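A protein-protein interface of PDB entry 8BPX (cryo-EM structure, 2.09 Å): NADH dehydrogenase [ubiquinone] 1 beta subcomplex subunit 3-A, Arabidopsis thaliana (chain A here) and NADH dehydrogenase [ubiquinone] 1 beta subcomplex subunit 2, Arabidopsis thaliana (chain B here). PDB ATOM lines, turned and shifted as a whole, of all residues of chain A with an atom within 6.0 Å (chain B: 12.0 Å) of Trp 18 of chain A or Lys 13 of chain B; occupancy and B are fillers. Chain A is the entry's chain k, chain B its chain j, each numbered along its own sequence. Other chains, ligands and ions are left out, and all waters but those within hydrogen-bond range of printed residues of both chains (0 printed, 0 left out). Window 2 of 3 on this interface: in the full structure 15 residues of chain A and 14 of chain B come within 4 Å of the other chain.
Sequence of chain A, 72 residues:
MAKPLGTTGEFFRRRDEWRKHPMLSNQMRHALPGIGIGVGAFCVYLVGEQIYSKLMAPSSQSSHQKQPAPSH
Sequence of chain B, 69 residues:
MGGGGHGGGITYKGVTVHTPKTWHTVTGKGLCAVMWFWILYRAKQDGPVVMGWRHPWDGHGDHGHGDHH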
ATOM      1  N   ARG A  14      -1.365   6.270  -1.151  1.00  0.00           N
ATOM      2  CA  ARG A  14      -2.015   5.627  -2.286  1.00  0.00           C
ATOM      3  C   ARG A  14      -3.529   5.659  -2.143  1.00  0.00           C
ATOM      4  O   ARG A  14      -4.245   5.900  -3.121  1.00  0.00           O
ATOM      5  CB  ARG A  14      -1.523   4.189  -2.425  1.00  0.00           C
ATOM      6  CG  ARG A  14      -0.312   4.043  -3.307  1.00  0.00           C
ATOM      7  CD  ARG A  14      -0.164   2.632  -3.818  1.00  0.00           C
ATOM      8  NE  ARG A  14       1.233   2.226  -3.900  1.00  0.00           N
ATOM      9  CZ  ARG A  14       1.657   0.976  -3.796  1.00  0.00           C
ATOM     10  NH1 ARG A  14       0.815  -0.025  -3.606  1.00  0.00           N
ATOM     11  NH2 ARG A  14       2.958   0.724  -3.893  1.00  0.00           N
ATOM     12  N   ARG A  15      -4.038   5.411  -0.933  1.00  0.00           N
ATOM     13  CA  ARG A  15      -5.483   5.453  -0.734  1.00  0.00           C
ATOM     14  C   ARG A  15      -6.056   6.855  -0.893  1.00  0.00           C
ATOM     15  O   ARG A  15      -7.246   6.990  -1.191  1.00  0.00           O
ATOM     16  CB  ARG A  15      -5.851   4.903   0.646  1.00  0.00           C
ATOM     17  CG  ARG A  15      -5.457   3.452   0.874  1.00  0.00           C
ATOM     18  CD  ARG A  15      -6.211   2.497  -0.028  1.00  0.00           C
ATOM     19  NE  ARG A  15      -7.634   2.800  -0.094  1.00  0.00           N
ATOM     20  CZ  ARG A  15      -8.382   2.670  -1.179  1.00  0.00           C
ATOM     21  NH1 ARG A  15      -7.879   2.214  -2.314  1.00  0.00           N
ATOM     22  NH2 ARG A  15      -9.668   2.993  -1.122  1.00  0.00           N
ATOM     23  N   ASP A  16      -5.244   7.893  -0.712  1.00  0.00           N
ATOM     24  CA  ASP A  16      -5.709   9.272  -0.756  1.00  0.00           C
ATOM     25  C   ASP A  16      -5.655   9.880  -2.154  1.00  0.00           C
ATOM     26  O   ASP A  16      -5.727  11.104  -2.281  1.00  0.00           O
ATOM     27  CB  ASP A  16      -4.885  10.141   0.201  1.00  0.00           C
ATOM     28  CG  ASP A  16      -5.354  10.046   1.641  1.00  0.00           C
ATOM     29  OD1 ASP A  16      -6.574   9.952   1.871  1.00  0.00           O
ATOM     30  OD2 ASP A  16      -4.503  10.087   2.546  1.00  0.00           O
ATOM     31  N   GLU A  17      -5.536   9.057  -3.200  1.00  0.00           N
ATOM     32  CA  GLU A  17      -5.378   9.595  -4.549  1.00  0.00           C
ATOM     33  C   GLU A  17      -6.582  10.425  -4.978  1.00  0.00           C
ATOM     34  O   GLU A  17      -6.423  11.419  -5.695  1.00  0.00           O
ATOM     35  CB  GLU A  17      -5.137   8.462  -5.542  1.00  0.00           C
ATOM     36  CG  GLU A  17      -3.688   8.056  -5.676  1.00  0.00           C
ATOM     37  CD  GLU A  17      -3.525   6.647  -6.210  1.00  0.00           C
ATOM     38  OE1 GLU A  17      -2.708   5.885  -5.655  1.00  0.00           O
ATOM     39  OE2 GLU A  17      -4.219   6.300  -7.190  1.00  0.00           O
ATOM     40  N   TRP A  18      -7.784  10.046  -4.542  1.00  0.00           N
ATOM     41  CA  TRP A  18      -8.983  10.789  -4.909  1.00  0.00           C
ATOM     42  C   TRP A  18      -8.967  12.217  -4.382  1.00  0.00           C
ATOM     43  O   TRP A  18      -9.705  13.063  -4.893  1.00  0.00           O
ATOM     44  CB  TRP A  18     -10.227  10.056  -4.402  1.00  0.00           C
ATOM     45  CG  TRP A  18     -10.381  10.074  -2.913  1.00  0.00           C
ATOM     46  CD1 TRP A  18      -9.932   9.136  -2.035  1.00  0.00           C
ATOM     47  CD2 TRP A  18     -11.019  11.085  -2.128  1.00  0.00           C
ATOM     48  NE1 TRP A  18     -10.255   9.494  -0.754  1.00  0.00           N
ATOM     49  CE2 TRP A  18     -10.926  10.686  -0.780  1.00  0.00           C
ATOM     50  CE3 TRP A  18     -11.663  12.288  -2.431  1.00  0.00           C
ATOM     51  CZ2 TRP A  18     -11.449  11.442   0.260  1.00  0.00           C
ATOM     52  CZ3 TRP A  18     -12.183  13.037  -1.397  1.00  0.00           C
ATOM     53  CH2 TRP A  18     -12.073  12.613  -0.068  1.00  0.00           C
ATOM     54  N   ARG A  19      -8.139  12.507  -3.382  1.00  0.00           N
ATOM     55  CA  ARG A  19      -8.051  13.854  -2.838  1.00  0.00           C
ATOM     56  C   ARG A  19      -7.383  14.832  -3.794  1.00  0.00           C
ATOM     57  O   ARG A  19      -7.393  16.038  -3.528  1.00  0.00           O
ATOM     58  CB  ARG A  19      -7.311  13.822  -1.505  1.00  0.00           C
ATOM     59  CG  ARG A  19      -8.196  13.379  -0.356  1.00  0.00           C
ATOM     60  CD  ARG A  19      -7.392  13.035   0.873  1.00  0.00           C
ATOM     61  NE  ARG A  19      -8.010  11.949   1.619  1.00  0.00           N
ATOM     62  CZ  ARG A  19      -8.862  12.120   2.617  1.00  0.00           C
ATOM     63  NH1 ARG A  19      -9.250  13.328   2.994  1.00  0.00           N
ATOM     64  NH2 ARG A  19      -9.350  11.055   3.244  1.00  0.00           N
ATOM     65  N   LYS A  20      -6.806  14.349  -4.892  1.00  0.00           N
ATOM     66  CA  LYS A  20      -6.361  15.205  -5.981  1.00  0.00           C
ATOM     67  C   LYS A  20      -7.498  15.557  -6.930  1.00  0.00           C
ATOM     68  O   LYS A  20      -7.239  15.949  -8.072  1.00  0.00           O
ATOM     69  CB  LYS A  20      -5.219  14.539  -6.752  1.00  0.00           C
ATOM     70  CG  LYS A  20      -4.071  14.035  -5.902  1.00  0.00           C
ATOM     71  CD  LYS A  20      -3.701  15.014  -4.801  1.00  0.00           C
ATOM     72  CE  LYS A  20      -2.403  14.614  -4.121  1.00  0.00           C
ATOM     73  NZ  LYS A  20      -1.465  15.762  -3.967  1.00  0.00           N
ATOM     74  N   HIS A  21      -8.741  15.422  -6.475  1.00  0.00           N
ATOM     75  CA  HIS A  21      -9.898  15.799  -7.272  1.00  0.00           C
ATOM     76  C   HIS A  21      -9.751  17.245  -7.741  1.00  0.00           C
ATOM     77  O   HIS A  21      -9.345  18.109  -6.955  1.00  0.00           O
ATOM     78  CB  HIS A  21     -11.180  15.651  -6.445  1.00  0.00           C
ATOM     79  CG  HIS A  21     -12.390  15.292  -7.248  1.00  0.00           C
ATOM     80  ND1 HIS A  21     -13.011  16.184  -8.098  1.00  0.00           N
ATOM     81  CD2 HIS A  21     -13.123  14.156  -7.298  1.00  0.00           C
ATOM     82  CE1 HIS A  21     -14.056  15.602  -8.659  1.00  0.00           C
ATOM     83  NE2 HIS A  21     -14.147  14.369  -8.190  1.00  0.00           N
ATOM     84  N   LEU A  24     -11.761  19.718  -5.631  1.00  0.00           N
ATOM     85  CA  LEU A  24     -11.521  19.611  -4.201  1.00  0.00           C
ATOM     86  C   LEU A  24     -10.178  20.196  -3.796  1.00  0.00           C
ATOM     87  O   LEU A  24      -9.910  20.323  -2.596  1.00  0.00           O
ATOM     88  CB  LEU A  24     -11.587  18.142  -3.762  1.00  0.00           C
ATOM     89  CG  LEU A  24     -12.968  17.493  -3.707  1.00  0.00           C
ATOM     90  CD1 LEU A  24     -12.976  16.344  -2.717  1.00  0.00           C
ATOM     91  CD2 LEU A  24     -14.044  18.516  -3.364  1.00  0.00           C
ATOM     92  N   GLY B   9     -22.374  16.211 -11.863  1.00  0.00           N
ATOM     93  CA  GLY B   9     -21.123  16.100 -11.137  1.00  0.00           C
ATOM     94  C   GLY B   9     -19.991  15.435 -11.900  1.00  0.00           C
ATOM     95  O   GLY B   9     -20.210  14.807 -12.936  1.00  0.00           O
ATOM     96  N   ILE B  10     -18.773  15.576 -11.378  1.00  0.00           N
ATOM     97  CA  ILE B  10     -17.576  14.997 -11.975  1.00  0.00           C
ATOM     98  C   ILE B  10     -17.054  13.900 -11.058  1.00  0.00           C
ATOM     99  O   ILE B  10     -16.875  14.119  -9.852  1.00  0.00           O
ATOM    100  CB  ILE B  10     -16.504  16.071 -12.220  1.00  0.00           C
ATOM    101  CG1 ILE B  10     -17.083  17.206 -13.068  1.00  0.00           C
ATOM    102  CG2 ILE B  10     -15.286  15.472 -12.903  1.00  0.00           C
ATOM    103  CD1 ILE B  10     -16.904  18.571 -12.464  1.00  0.00           C
ATOM    104  N   THR B  11     -16.810  12.721 -11.623  1.00  0.00           N
ATOM    105  CA  THR B  11     -16.420  11.542 -10.858  1.00  0.00           C
ATOM    106  C   THR B  11     -14.940  11.265 -11.084  1.00  0.00           C
ATOM    107  O   THR B  11     -14.508  11.071 -12.225  1.00  0.00           O
ATOM    108  CB  THR B  11     -17.257  10.331 -11.260  1.00  0.00           C
ATOM    109  OG1 THR B  11     -18.641  10.597 -10.995  1.00  0.00           O
ATOM    110  CG2 THR B  11     -16.828   9.106 -10.471  1.00  0.00           C
ATOM    111  N   TYR B  12     -14.171  11.242  -9.999  1.00  0.00           N
ATOM    112  CA  TYR B  12     -12.737  10.973 -10.041  1.00  0.00           C
ATOM    113  C   TYR B  12     -12.434   9.813  -9.104  1.00  0.00           C
ATOM    114  O   TYR B  12     -12.497   9.971  -7.879  1.00  0.00           O
ATOM    115  CB  TYR B  12     -11.930  12.208  -9.648  1.00  0.00           C
ATOM    116  CG  TYR B  12     -10.476  12.145 -10.043  1.00  0.00           C
ATOM    117  CD1 TYR B  12     -10.004  11.142 -10.874  1.00  0.00           C
ATOM    118  CD2 TYR B  12      -9.568  13.062  -9.544  1.00  0.00           C
ATOM    119  CE1 TYR B  12      -8.672  11.078 -11.225  1.00  0.00           C
ATOM    120  CE2 TYR B  12      -8.236  13.005  -9.883  1.00  0.00           C
ATOM    121  CZ  TYR B  12      -7.791  12.013 -10.726  1.00  0.00           C
ATOM    122  OH  TYR B  12      -6.461  11.955 -11.066  1.00  0.00           O
ATOM    123  N   LYS B  13     -12.089   8.662  -9.687  1.00  0.00           N
ATOM    124  CA  LYS B  13     -11.763   7.423  -8.985  1.00  0.00           C
ATOM    125  C   LYS B  13     -12.650   7.174  -7.768  1.00  0.00           C
ATOM    126  O   LYS B  13     -12.168   7.131  -6.631  1.00  0.00           O
ATOM    127  CB  LYS B  13     -10.275   7.362  -8.597  1.00  0.00           C
ATOM    128  CG  LYS B  13      -9.653   8.577  -7.942  1.00  0.00           C
ATOM    129  CD  LYS B  13      -8.215   8.276  -7.557  1.00  0.00           C
ATOM    130  CE  LYS B  13      -7.205   8.808  -8.559  1.00  0.00           C
ATOM    131  NZ  LYS B  13      -6.949  10.262  -8.396  1.00  0.00           N
ATOM    132  N   GLY B  14     -13.936   6.999  -8.003  1.00  0.00           N
ATOM    133  CA  GLY B  14     -14.882   6.669  -6.946  1.00  0.00           C
ATOM    134  C   GLY B  14     -15.646   7.822  -6.352  1.00  0.00           C
ATOM    135  O   GLY B  14     -16.863   7.749  -6.201  1.00  0.00           O
ATOM    136  N   VAL B  15     -14.948   8.892  -6.005  1.00  0.00           N
ATOM    137  CA  VAL B  15     -15.579  10.032  -5.357  1.00  0.00           C
ATOM    138  C   VAL B  15     -16.208  10.932  -6.412  1.00  0.00           C
ATOM    139  O   VAL B  15     -15.559  11.320  -7.389  1.00  0.00           O
ATOM    140  CB  VAL B  15     -14.561  10.795  -4.497  1.00  0.00           C
ATOM    141  CG1 VAL B  15     -15.178  12.051  -3.947  1.00  0.00           C
ATOM    142  CG2 VAL B  15     -14.062   9.899  -3.371  1.00  0.00           C
ATOM    143  N   THR B  16     -17.479  11.265  -6.215  1.00  0.00           N
ATOM    144  CA  THR B  16     -18.228  12.121  -7.120  1.00  0.00           C
ATOM    145  C   THR B  16     -18.558  13.428  -6.414  1.00  0.00           C
ATOM    146  O   THR B  16     -19.124  13.420  -5.316  1.00  0.00           O
ATOM    147  CB  THR B  16     -19.513  11.433  -7.585  1.00  0.00           C
ATOM    148  OG1 THR B  16     -19.209  10.538  -8.663  1.00  0.00           O
ATOM    149  CG2 THR B  16     -20.530  12.453  -8.059  1.00  0.00           C
ATOM    150  N   VAL B  17     -18.205  14.545  -7.040  1.00  0.00           N
ATOM    151  CA  VAL B  17     -18.470  15.869  -6.491  1.00  0.00           C
ATOM    152  C   VAL B  17     -19.484  16.559  -7.389  1.00  0.00           C
ATOM    153  O   VAL B  17     -19.282  16.654  -8.605  1.00  0.00           O
ATOM    154  CB  VAL B  17     -17.182  16.700  -6.362  1.00  0.00           C
ATOM    155  CG1 VAL B  17     -17.412  17.892  -5.443  1.00  0.00           C
ATOM    156  CG2 VAL B  17     -16.046  15.842  -5.851  1.00  0.00           C
ATOM    157  N   HIS B  18     -20.580  17.017  -6.793  1.00  0.00           N
ATOM    158  CA  HIS B  18     -21.640  17.692  -7.524  1.00  0.00           C
ATOM    159  C   HIS B  18     -21.334  19.175  -7.663  1.00  0.00           C
ATOM    160  O   HIS B  18     -20.926  19.831  -6.701  1.00  0.00           O
ATOM    161  CB  HIS B  18     -22.989  17.512  -6.826  1.00  0.00           C
ATOM    162  CG  HIS B  18     -23.215  16.138  -6.281  1.00  0.00           C
ATOM    163  ND1 HIS B  18     -23.741  15.117  -7.042  1.00  0.00           N
ATOM    164  CD2 HIS B  18     -23.007  15.620  -5.048  1.00  0.00           C
ATOM    165  CE1 HIS B  18     -23.837  14.027  -6.304  1.00  0.00           C
ATOM    166  NE2 HIS B  18     -23.397  14.304  -5.090  1.00  0.00           N
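O of Val 15 of chain B lies within hydrogen-bond range of NE2 of His 21 of chain A (3.5 Å).
The backbone carbonyl oxygen of Ile 10 of chain B lies within hydrogen-bond range of a ring nitrogen (NE2) of His 21 of chain A (3.2 Å).
The side-chain amino group of Lys 13 of chain B sits at hydrogen-bond distance from the backbone carbonyl oxygen of Glu 17 of chain A (3.0 Å).
Trp 18 of chain A touches Lys 13 of chain B.
Val 15 of chain B touches Trp 18 of chain A (CG2 to CD2, 3.5 Å).
Lys 20 of chain A touches Tyr 12 of chain B (O to CE2, 3.6 Å).
Tyr 12 of chain B touches His 21 of chain A.
His 21 of chain A touches Val 17 of chain B (NE2 to CG2, 3.4 Å).
Of the 9 printed residues of chain A, 4 touch a printed residue of chain B.
Printed residues of chain A that touch a printed residue of chain B: Glu 17, Trp 18, Lys 20 and His 21.
Hydrophobic or aromatic side chains of chain A within 4 Å of the printed part of chain B: Trp 18 and His 21.
Hydrophobic or aromatic side chains of chain B that line the printed part of chain A: Tyr 12, Val 15 and Val 17.
Among the printed residues, 8 pairs touch across the chains.
The side-chain amino group (NZ) of Lys 13 of chain B lies close to the side-chain hydroxyl (OH) of Tyr 12 of chain B, at 3.2 Å.
N of Ile 10 of chain B sits at hydrogen-bond distance from O of Val 17 of chain B, at 3.0 Å.
Arg 14 of chain A touches none of the printed residues of chain B.
Of chain B, only Lys 13 (3.5 Å) and Val 15 (3.5 Å) come within 4 Å of Trp 18 of chain A.
No residue of chain B comes within 4 Å of Arg 19 of chain A.
Of the printed residues of chain B, His 21 of chain A touches Ile 10, Tyr 12, Val 15 and Val 17.
Leu 24 of chain A touches none of the printed residues of chain B.
Printed residues of chain A within 4 Å of Ile 10 of chain B: His 21 (3.2 Å).
Printed residues of chain A within 4 Å of Val 15 of chain B: Trp 18 (3.5 Å) and His 21 (3.5 Å).
Printed residues of chain A within 4 Å of Val 17 of chain B: His 21.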
